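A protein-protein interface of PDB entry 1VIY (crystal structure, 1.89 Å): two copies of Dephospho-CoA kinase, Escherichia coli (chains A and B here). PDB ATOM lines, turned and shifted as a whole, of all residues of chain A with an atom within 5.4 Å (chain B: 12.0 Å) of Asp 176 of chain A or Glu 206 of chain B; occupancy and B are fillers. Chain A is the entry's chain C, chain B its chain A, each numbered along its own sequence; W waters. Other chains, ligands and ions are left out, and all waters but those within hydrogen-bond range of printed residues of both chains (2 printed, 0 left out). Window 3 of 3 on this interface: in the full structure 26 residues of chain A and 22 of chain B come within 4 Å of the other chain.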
ATOM      1  N   VAL A 132       2.944  27.451  33.995  1.00  0.00           N
ATOM      2  CA  VAL A 132       2.781  26.144  33.376  1.00  0.00           C
ATOM      3  C   VAL A 132       2.273  26.448  31.979  1.00  0.00           C
ATOM      4  O   VAL A 132       1.203  27.006  31.815  1.00  0.00           O
ATOM      5  CB  VAL A 132       1.684  25.290  34.061  1.00  0.00           C
ATOM      6  CG1 VAL A 132       1.682  23.899  33.470  1.00  0.00           C
ATOM      7  CG2 VAL A 132       1.853  25.242  35.564  1.00  0.00           C
ATOM      8  N   ASP A 133       3.028  26.055  30.974  1.00  0.00           N
ATOM      9  CA  ASP A 133       2.716  26.471  29.628  1.00  0.00           C
ATOM     10  C   ASP A 133       2.328  25.272  28.782  1.00  0.00           C
ATOM     11  O   ASP A 133       2.870  24.178  28.973  1.00  0.00           O
ATOM     12  CB  ASP A 133       3.947  27.194  29.057  1.00  0.00           C
ATOM     13  CG  ASP A 133       3.737  27.660  27.636  1.00  0.00           C
ATOM     14  OD1 ASP A 133       2.959  28.620  27.424  1.00  0.00           O
ATOM     15  OD2 ASP A 133       4.321  27.121  26.686  1.00  0.00           O
ATOM     16  N   VAL A 134       1.380  25.492  27.861  1.00  0.00           N
ATOM     17  CA  VAL A 134       0.933  24.501  26.900  1.00  0.00           C
ATOM     18  C   VAL A 134       0.442  25.241  25.632  1.00  0.00           C
ATOM     19  O   VAL A 134       0.274  26.473  25.641  1.00  0.00           O
ATOM     20  CB  VAL A 134      -0.245  23.631  27.471  1.00  0.00           C
ATOM     21  CG1 VAL A 134       0.212  22.704  28.665  1.00  0.00           C
ATOM     22  CG2 VAL A 134      -1.418  24.498  27.886  1.00  0.00           C
ATOM     23  N   SER A 135       0.249  24.503  24.537  1.00  0.00           N
ATOM     24  CA  SER A 135      -0.350  25.097  23.336  1.00  0.00           C
ATOM     25  C   SER A 135      -1.835  25.385  23.606  1.00  0.00           C
ATOM     26  O   SER A 135      -2.460  24.673  24.391  1.00  0.00           O
ATOM     27  CB  SER A 135      -0.215  24.147  22.150  1.00  0.00           C
ATOM     28  OG  SER A 135      -0.969  22.973  22.398  1.00  0.00           O
ATOM     29  N   THR A 138      -3.611  22.155  23.138  1.00  0.00           N
ATOM     30  CA  THR A 138      -3.676  21.380  24.400  1.00  0.00           C
ATOM     31  C   THR A 138      -4.728  21.860  25.381  1.00  0.00           C
ATOM     32  O   THR A 138      -5.471  21.040  25.964  1.00  0.00           O
ATOM     33  CB  THR A 138      -2.314  21.362  25.077  1.00  0.00           C
ATOM     34  OG1 THR A 138      -1.421  20.578  24.281  1.00  0.00           O
ATOM     35  CG2 THR A 138      -2.391  20.638  26.498  1.00  0.00           C
ATOM     36  N   ARG A 164      -1.370  33.486  26.215  1.00  0.00           N
ATOM     37  CA  ARG A 164      -0.168  32.678  26.509  1.00  0.00           C
ATOM     38  C   ARG A 164       1.075  33.592  26.590  1.00  0.00           C
ATOM     39  O   ARG A 164       1.953  33.462  27.483  1.00  0.00           O
ATOM     40  CB  ARG A 164      -0.007  31.644  25.394  1.00  0.00           C
ATOM     41  CG  ARG A 164       1.160  30.686  25.543  1.00  0.00           C
ATOM     42  CD  ARG A 164       1.407  29.878  24.290  1.00  0.00           C
ATOM     43  NE  ARG A 164       2.333  28.794  24.572  1.00  0.00           N
ATOM     44  CZ  ARG A 164       2.646  27.834  23.710  1.00  0.00           C
ATOM     45  NH1 ARG A 164       2.202  27.915  22.460  1.00  0.00           N
ATOM     46  NH2 ARG A 164       3.476  26.839  24.083  1.00  0.00           N
ATOM     47  N   VAL A 174       9.445  28.606  33.360  1.00  0.00           N
ATOM     48  CA  VAL A 174       8.383  28.076  32.534  1.00  0.00           C
ATOM     49  C   VAL A 174       8.507  26.559  32.519  1.00  0.00           C
ATOM     50  O   VAL A 174       9.575  26.010  32.190  1.00  0.00           O
ATOM     51  CB  VAL A 174       8.440  28.645  31.092  1.00  0.00           C
ATOM     52  CG1 VAL A 174       7.281  28.069  30.212  1.00  0.00           C
ATOM     53  CG2 VAL A 174       8.436  30.189  31.106  1.00  0.00           C
ATOM     54  N   ILE A 175       7.416  25.883  32.844  1.00  0.00           N
ATOM     55  CA  ILE A 175       7.377  24.416  32.718  1.00  0.00           C
ATOM     56  C   ILE A 175       6.412  23.979  31.622  1.00  0.00           C
ATOM     57  O   ILE A 175       5.225  24.303  31.664  1.00  0.00           O
ATOM     58  CB  ILE A 175       7.019  23.770  34.079  1.00  0.00           C
ATOM     59  CG1 ILE A 175       6.908  22.247  33.979  1.00  0.00           C
ATOM     60  CG2 ILE A 175       5.737  24.340  34.633  1.00  0.00           C
ATOM     61  CD1 ILE A 175       7.259  21.606  35.351  1.00  0.00           C
ATOM     62  N   ASP A 176       6.911  23.236  30.651  1.00  0.00           N
ATOM     63  CA  ASP A 176       6.049  22.731  29.562  1.00  0.00           C
ATOM     64  C   ASP A 176       5.159  21.600  30.110  1.00  0.00           C
ATOM     65  O   ASP A 176       5.680  20.638  30.715  1.00  0.00           O
ATOM     66  CB  ASP A 176       6.919  22.230  28.402  1.00  0.00           C
ATOM     67  CG  ASP A 176       6.087  21.665  27.234  1.00  0.00           C
ATOM     68  OD1 ASP A 176       5.423  20.645  27.391  1.00  0.00           O
ATOM     69  OD2 ASP A 176       5.997  22.212  26.138  1.00  0.00           O
ATOM     70  N   ASN A 177       3.833  21.700  29.938  1.00  0.00           N
ATOM     71  CA  ASN A 177       2.954  20.590  30.349  1.00  0.00           C
ATOM     72  C   ASN A 177       2.111  20.009  29.194  1.00  0.00           C
ATOM     73  O   ASN A 177       0.913  19.728  29.355  1.00  0.00           O
ATOM     74  CB  ASN A 177       2.078  20.950  31.564  1.00  0.00           C
ATOM     75  CG  ASN A 177       1.351  19.737  32.148  1.00  0.00           C
ATOM     76  OD1 ASN A 177       1.861  18.623  32.119  1.00  0.00           O
ATOM     77  ND2 ASN A 177       0.148  19.955  32.669  1.00  0.00           N
ATOM     78  N   ASN A 178       2.727  19.840  28.032  1.00  0.00           N
ATOM     79  CA  ASN A 178       1.954  19.405  26.864  1.00  0.00           C
ATOM     80  C   ASN A 178       1.666  17.874  26.914  1.00  0.00           C
ATOM     81  O   ASN A 178       0.600  17.412  26.463  1.00  0.00           O
ATOM     82  CB  ASN A 178       2.624  19.857  25.554  1.00  0.00           C
ATOM     83  CG  ASN A 178       2.315  21.337  25.187  1.00  0.00           C
ATOM     84  OD1 ASN A 178       1.150  21.733  24.943  1.00  0.00           O
ATOM     85  ND2 ASN A 178       3.364  22.150  25.152  1.00  0.00           N
ATOM     86  N   GLY A 179       2.578  17.105  27.526  1.00  0.00           N
ATOM     87  CA  GLY A 179       2.421  15.657  27.622  1.00  0.00           C
ATOM     88  C   GLY A 179       1.752  15.060  28.853  1.00  0.00           C
ATOM     89  O   GLY A 179       0.853  15.644  29.466  1.00  0.00           O
ATOM     90  N   ILE A 184       6.765  16.100  33.568  1.00  0.00           N
ATOM     91  CA  ILE A 184       7.179  17.343  34.231  1.00  0.00           C
ATOM     92  C   ILE A 184       8.220  17.110  35.332  1.00  0.00           C
ATOM     93  O   ILE A 184       8.764  18.072  35.890  1.00  0.00           O
ATOM     94  CB  ILE A 184       5.941  18.086  34.801  1.00  0.00           C
ATOM     95  CG1 ILE A 184       5.297  17.286  35.960  1.00  0.00           C
ATOM     96  CG2 ILE A 184       4.976  18.408  33.666  1.00  0.00           C
ATOM     97  CD1 ILE A 184       4.246  18.058  36.799  1.00  0.00           C
ATOM     98  N   ASP A 187      11.851  18.866  35.333  1.00  0.00           N
ATOM     99  CA  ASP A 187      11.753  20.297  35.661  1.00  0.00           C
ATOM    100  C   ASP A 187      11.349  20.524  37.098  1.00  0.00           C
ATOM    101  O   ASP A 187      11.871  21.406  37.759  1.00  0.00           O
ATOM    102  CB  ASP A 187      10.701  20.984  34.792  1.00  0.00           C
ATOM    103  CG  ASP A 187      11.117  21.047  33.353  1.00  0.00           C
ATOM    104  OD1 ASP A 187      12.291  21.371  33.074  1.00  0.00           O
ATOM    105  OD2 ASP A 187      10.335  20.759  32.451  1.00  0.00           O
ATOM    106  N   GLN B 197       2.814  34.086   9.561  1.00  0.00           N
ATOM    107  CA  GLN B 197       3.464  32.845  10.054  1.00  0.00           C
ATOM    108  C   GLN B 197       3.057  32.539  11.493  1.00  0.00           C
ATOM    109  O   GLN B 197       2.592  31.430  11.797  1.00  0.00           O
ATOM    110  CB  GLN B 197       4.986  32.911   9.902  1.00  0.00           C
ATOM    111  CG  GLN B 197       5.743  31.693  10.534  1.00  0.00           C
ATOM    112  CD  GLN B 197       5.489  30.376   9.828  1.00  0.00           C
ATOM    113  OE1 GLN B 197       5.584  30.304   8.606  1.00  0.00           O
ATOM    114  NE2 GLN B 197       5.178  29.323  10.593  1.00  0.00           N
ATOM    115  N   LEU B 198       3.165  33.529  12.388  1.00  0.00           N
ATOM    116  CA  LEU B 198       2.721  33.299  13.780  1.00  0.00           C
ATOM    117  C   LEU B 198       1.260  32.918  13.871  1.00  0.00           C
ATOM    118  O   LEU B 198       0.891  32.026  14.640  1.00  0.00           O
ATOM    119  CB  LEU B 198       2.945  34.547  14.648  1.00  0.00           C
ATOM    120  CG  LEU B 198       4.365  35.030  14.781  1.00  0.00           C
ATOM    121  CD1 LEU B 198       4.355  36.479  15.293  1.00  0.00           C
ATOM    122  CD2 LEU B 198       5.069  34.083  15.773  1.00  0.00           C
ATOM    123  N   ALA B 199       0.395  33.603  13.119  1.00  0.00           N
ATOM    124  CA  ALA B 199      -1.036  33.243  13.071  1.00  0.00           C
ATOM    125  C   ALA B 199      -1.308  31.791  12.632  1.00  0.00           C
ATOM    126  O   ALA B 199      -2.219  31.109  13.160  1.00  0.00           O
ATOM    127  CB  ALA B 199      -1.779  34.187  12.139  1.00  0.00           C
ATOM    128  N   SER B 200      -0.509  31.303  11.686  1.00  0.00           N
ATOM    129  CA  SER B 200      -0.713  29.972  11.118  1.00  0.00           C
ATOM    130  C   SER B 200      -0.276  28.892  12.101  1.00  0.00           C
ATOM    131  O   SER B 200      -0.746  27.750  12.031  1.00  0.00           O
ATOM    132  CB  SER B 200       0.094  29.825   9.830  1.00  0.00           C
ATOM    133  OG  SER B 200       1.472  29.621  10.153  1.00  0.00           O
ATOM    134  N   GLN B 201       0.604  29.259  13.030  1.00  0.00           N
ATOM    135  CA  GLN B 201       1.229  28.276  13.896  1.00  0.00           C
ATOM    136  C   GLN B 201       0.819  28.348  15.365  1.00  0.00           C
ATOM    137  O   GLN B 201       1.028  27.354  16.059  1.00  0.00           O
ATOM    138  CB  GLN B 201       2.760  28.341  13.812  1.00  0.00           C
ATOM    139  CG  GLN B 201       3.351  29.533  14.586  1.00  0.00           C
ATOM    140  CD  GLN B 201       4.826  29.764  14.304  1.00  0.00           C
ATOM    141  OE1 GLN B 201       5.309  29.436  13.224  1.00  0.00           O
ATOM    142  NE2 GLN B 201       5.546  30.337  15.284  1.00  0.00           N
ATOM    143  N   PHE B 202       0.236  29.460  15.848  1.00  0.00           N
ATOM    144  CA  PHE B 202       0.147  29.644  17.315  1.00  0.00           C
ATOM    145  C   PHE B 202      -0.734  28.627  18.058  1.00  0.00           C
ATOM    146  O   PHE B 202      -0.464  28.318  19.221  1.00  0.00           O
ATOM    147  CB  PHE B 202      -0.185  31.092  17.746  1.00  0.00           C
ATOM    148  CG  PHE B 202      -1.642  31.449  17.661  1.00  0.00           C
ATOM    149  CD1 PHE B 202      -2.382  31.724  18.817  1.00  0.00           C
ATOM    150  CD2 PHE B 202      -2.286  31.532  16.409  1.00  0.00           C
ATOM    151  CE1 PHE B 202      -3.733  32.075  18.734  1.00  0.00           C
ATOM    152  CE2 PHE B 202      -3.615  31.862  16.307  1.00  0.00           C
ATOM    153  CZ  PHE B 202      -4.364  32.132  17.477  1.00  0.00           C
ATOM    154  N   VAL B 203      -1.772  28.102  17.409  1.00  0.00           N
ATOM    155  CA  VAL B 203      -2.707  27.226  18.128  1.00  0.00           C
ATOM    156  C   VAL B 203      -2.061  25.891  18.545  1.00  0.00           C
ATOM    157  O   VAL B 203      -2.246  25.423  19.703  1.00  0.00           O
ATOM    158  CB  VAL B 203      -4.044  27.067  17.358  1.00  0.00           C
ATOM    159  CG1 VAL B 203      -4.889  25.883  17.858  1.00  0.00           C
ATOM    160  CG2 VAL B 203      -4.841  28.373  17.447  1.00  0.00           C
ATOM    161  N   SER B 204      -1.295  25.305  17.622  1.00  0.00           N
ATOM    162  CA  SER B 204      -0.643  23.996  17.850  1.00  0.00           C
ATOM    163  C   SER B 204       0.803  24.106  18.348  1.00  0.00           C
ATOM    164  O   SER B 204       1.397  23.095  18.738  1.00  0.00           O
ATOM    165  CB  SER B 204      -0.654  23.160  16.563  1.00  0.00           C
ATOM    166  OG  SER B 204      -0.045  23.919  15.513  1.00  0.00           O
ATOM    167  N   GLN B 205       1.359  25.324  18.387  1.00  0.00           N
ATOM    168  CA  GLN B 205       2.766  25.509  18.765  1.00  0.00           C
ATOM    169  C   GLN B 205       3.084  25.011  20.191  1.00  0.00           C
ATOM    170  O   GLN B 205       2.682  25.622  21.188  1.00  0.00           O
ATOM    171  CB  GLN B 205       3.157  26.983  18.631  1.00  0.00           C
ATOM    172  CG  GLN B 205       4.569  27.267  19.072  1.00  0.00           C
ATOM    173  CD  GLN B 205       5.080  28.611  18.651  1.00  0.00           C
ATOM    174  OE1 GLN B 205       4.325  29.475  18.182  1.00  0.00           O
ATOM    175  NE2 GLN B 205       6.376  28.801  18.804  1.00  0.00           N
ATOM    176  N   GLU B 206       3.834  23.919  20.274  1.00  0.00           N
ATOM    177  CA  GLU B 206       4.232  23.313  21.550  1.00  0.00           C
ATOM    178  C   GLU B 206       5.053  24.226  22.417  1.00  0.00           C
ATOM    179  O   GLU B 206       4.684  24.481  23.559  1.00  0.00           O
ATOM    180  CB  GLU B 206       5.052  22.046  21.300  1.00  0.00           C
ATOM    181  CG  GLU B 206       4.329  21.040  20.438  1.00  0.00           C
ATOM    182  CD  GLU B 206       3.915  19.832  21.219  1.00  0.00           C
ATOM    183  OE1 GLU B 206       3.202  19.998  22.240  1.00  0.00           O
ATOM    184  OE2 GLU B 206       4.315  18.724  20.810  1.00  0.00           O
ATOM    185  N   LYS B 207       6.183  24.673  21.879  1.00  0.00           N
ATOM    186  CA  LYS B 207       7.124  25.499  22.600  1.00  0.00           C
ATOM    187  C   LYS B 207       6.908  26.991  22.304  1.00  0.00           C
ATOM    188  O   LYS B 207       6.719  27.370  21.150  1.00  0.00           O
ATOM    189  CB  LYS B 207       8.559  25.105  22.222  1.00  0.00           C
ATOM    190  CG  LYS B 207       8.851  23.584  22.306  1.00  0.00           C
ATOM    191  CD  LYS B 207       9.308  23.121  23.689  1.00  0.00           C
ATOM    192  CE  LYS B 207       9.475  21.600  23.718  1.00  0.00           C
ATOM    193  NZ  LYS B 207      10.818  21.156  23.196  1.00  0.00           N
ATOM    194  N   PRO B 208       6.999  27.835  23.330  1.00  0.00           N
ATOM    195  CA  PRO B 208       6.829  29.288  23.148  1.00  0.00           C
ATOM    196  C   PRO B 208       7.847  29.833  22.137  1.00  0.00           C
ATOM    197  O   PRO B 208       8.968  29.327  22.088  1.00  0.00           O
ATOM    198  CB  PRO B 208       7.157  29.859  24.522  1.00  0.00           C
ATOM    199  CG  PRO B 208       7.086  28.731  25.475  1.00  0.00           C
ATOM    200  CD  PRO B 208       7.327  27.471  24.720  1.00  0.00           C
ATOM    201  N   GLU B 209       7.472  30.850  21.367  1.00  0.00           N
ATOM    202  CA  GLU B 209       8.319  31.395  20.288  1.00  0.00           C
ATOM    203  C   GLU B 209       9.291  30.385  19.640  1.00  0.00           C
ATOM    204  O   GLU B 209      10.513  30.403  19.879  1.00  0.00           O
ATOM    205  CB  GLU B 209       9.063  32.675  20.719  1.00  0.00           C
ATOM    206  CG  GLU B 209       9.745  32.635  22.078  1.00  0.00           C
ATOM    207  CD  GLU B 209       8.945  33.357  23.143  1.00  0.00           C
ATOM    208  OE1 GLU B 209       7.860  32.850  23.510  1.00  0.00           O
ATOM    209  OE2 GLU B 209       9.397  34.437  23.613  1.00  0.00           O
HETATM  210  O   HOH W   1       0.051  21.288  20.564  1.00  0.00           O
HETATM  211  O   HOH W   2       0.793  29.856  20.946  1.00  0.00           O
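The guanidinium group (NH1) of Arg 164 of chain A lies within hydrogen-bond range of the backbone carbonyl oxygen (O) of Gln 205 of chain B, 2.7 Å away.
O of Glu 206 of chain B sits at hydrogen-bond distance from NH2 of Arg 164 of chain A (2.7 Å).
O of Glu 206 of chain B sits at hydrogen-bond distance from ND2 of Asn 178 of chain A, at 3.1 Å.
The side-chain amide nitrogen (NE2) of Gln 205 of chain B sits close to the backbone NH (N) of Glu 209 of chain B.
The backbone NH of Asp 133 of chain A lies within hydrogen-bond range of the backbone carbonyl oxygen of Ile 175 of chain A, 2.9 Å away.
N of Asn 177 of chain A is in hydrogen-bond range of O of Asp 133 of chain A (2.8 Å).
N of Ser 135 of chain A is in hydrogen-bond range of OD1 of Asn 178 of chain A, at 2.9 Å.
The side-chain hydroxyl of Thr 138 of chain A is in hydrogen-bond range of the side-chain amide oxygen of Asn 178 of chain A (2.9 Å).
The side-chain carboxylate (OD2) of Asp 176 of chain A sits at hydrogen-bond distance from the side-chain amide nitrogen (ND2) of Asn 178 of chain A (2.8 Å).
Among the printed residues, pairs that only touch across the chains: Asp 133 of chain A with Pro 208 of chain B (3.4 Å), Ser 135 of chain A with Val 203 of chain B (3.4 Å), Ser 135 of chain A with Ser 204 of chain B (3.9 Å), Ser 135 of chain A with Gln 205 of chain B (3.4 Å), Arg 164 of chain A with Lys 207 of chain B (3.9 Å), Arg 164 of chain A with Pro 208 of chain B (3.7 Å) and Asp 176 of chain A with Glu 206 of chain B (3.7 Å).
Asp 176 of chain A touches just one residue of chain B: Glu 206.
Glu 206 of chain B touches three residues of chain A.
No residue of chain B comes within 4 Å of Val 132 of chain A.
Asp 133 of chain A touches one residue of chain B.
No residue of chain B comes within 4 Å of Val 134 of chain A.
No residue of chain B comes within 4 Å of Val 174 of chain A.
Asn 177 of chain A touches none of the printed residues of chain B.
Asn 178 of chain A touches just one residue of chain B: Glu 206 (3.1 Å).
No residue of chain B comes within 4 Å of Gly 179 of chain A.
No residue of chain B comes within 4 Å of Ile 184 of chain A.
Of the printed residues of chain B, Arg 164 of chain A touches Gln 205, Glu 206, Lys 207 and Pro 208.
Printed residues of chain A within 4 Å of Lys 207 of chain B: Arg 164 (3.9 Å).
The nearest residue of chain B that does not touch Asp 176 of chain A is Lys 207 of chain B (4.2 Å).
The nearest residue of chain A that does not touch Glu 206 of chain B is Asp 133 of chain A (4.1 Å).
Of the 13 printed residues of chain B, 6 touch a printed residue of chain A.
Hydrophobic or aromatic side chains of chain B within 4 Å of the printed part of chain A: Pro 208.
Printed residues of chain A that touch a printed residue of chain B: Asp 133, Ser 135, Arg 164, Asp 176 and Asn 178.
Among the printed residues, 10 pairs touch across the chains.
No position is printed for both chains.
Of the 10 pairs that touch across the chains among the printed residues, none has its exchanged pair printed and touching as well.
Water W2 bridges O of Phe 202 of chain B and NH1 of Arg 164 of chain A.
Water W1 bridges the side-chain hydroxyl (OG) of Ser 135 of chain A (2.7 Å) and the backbone carbonyl oxygen (O) of Ser 204 of chain B (2.9 Å).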
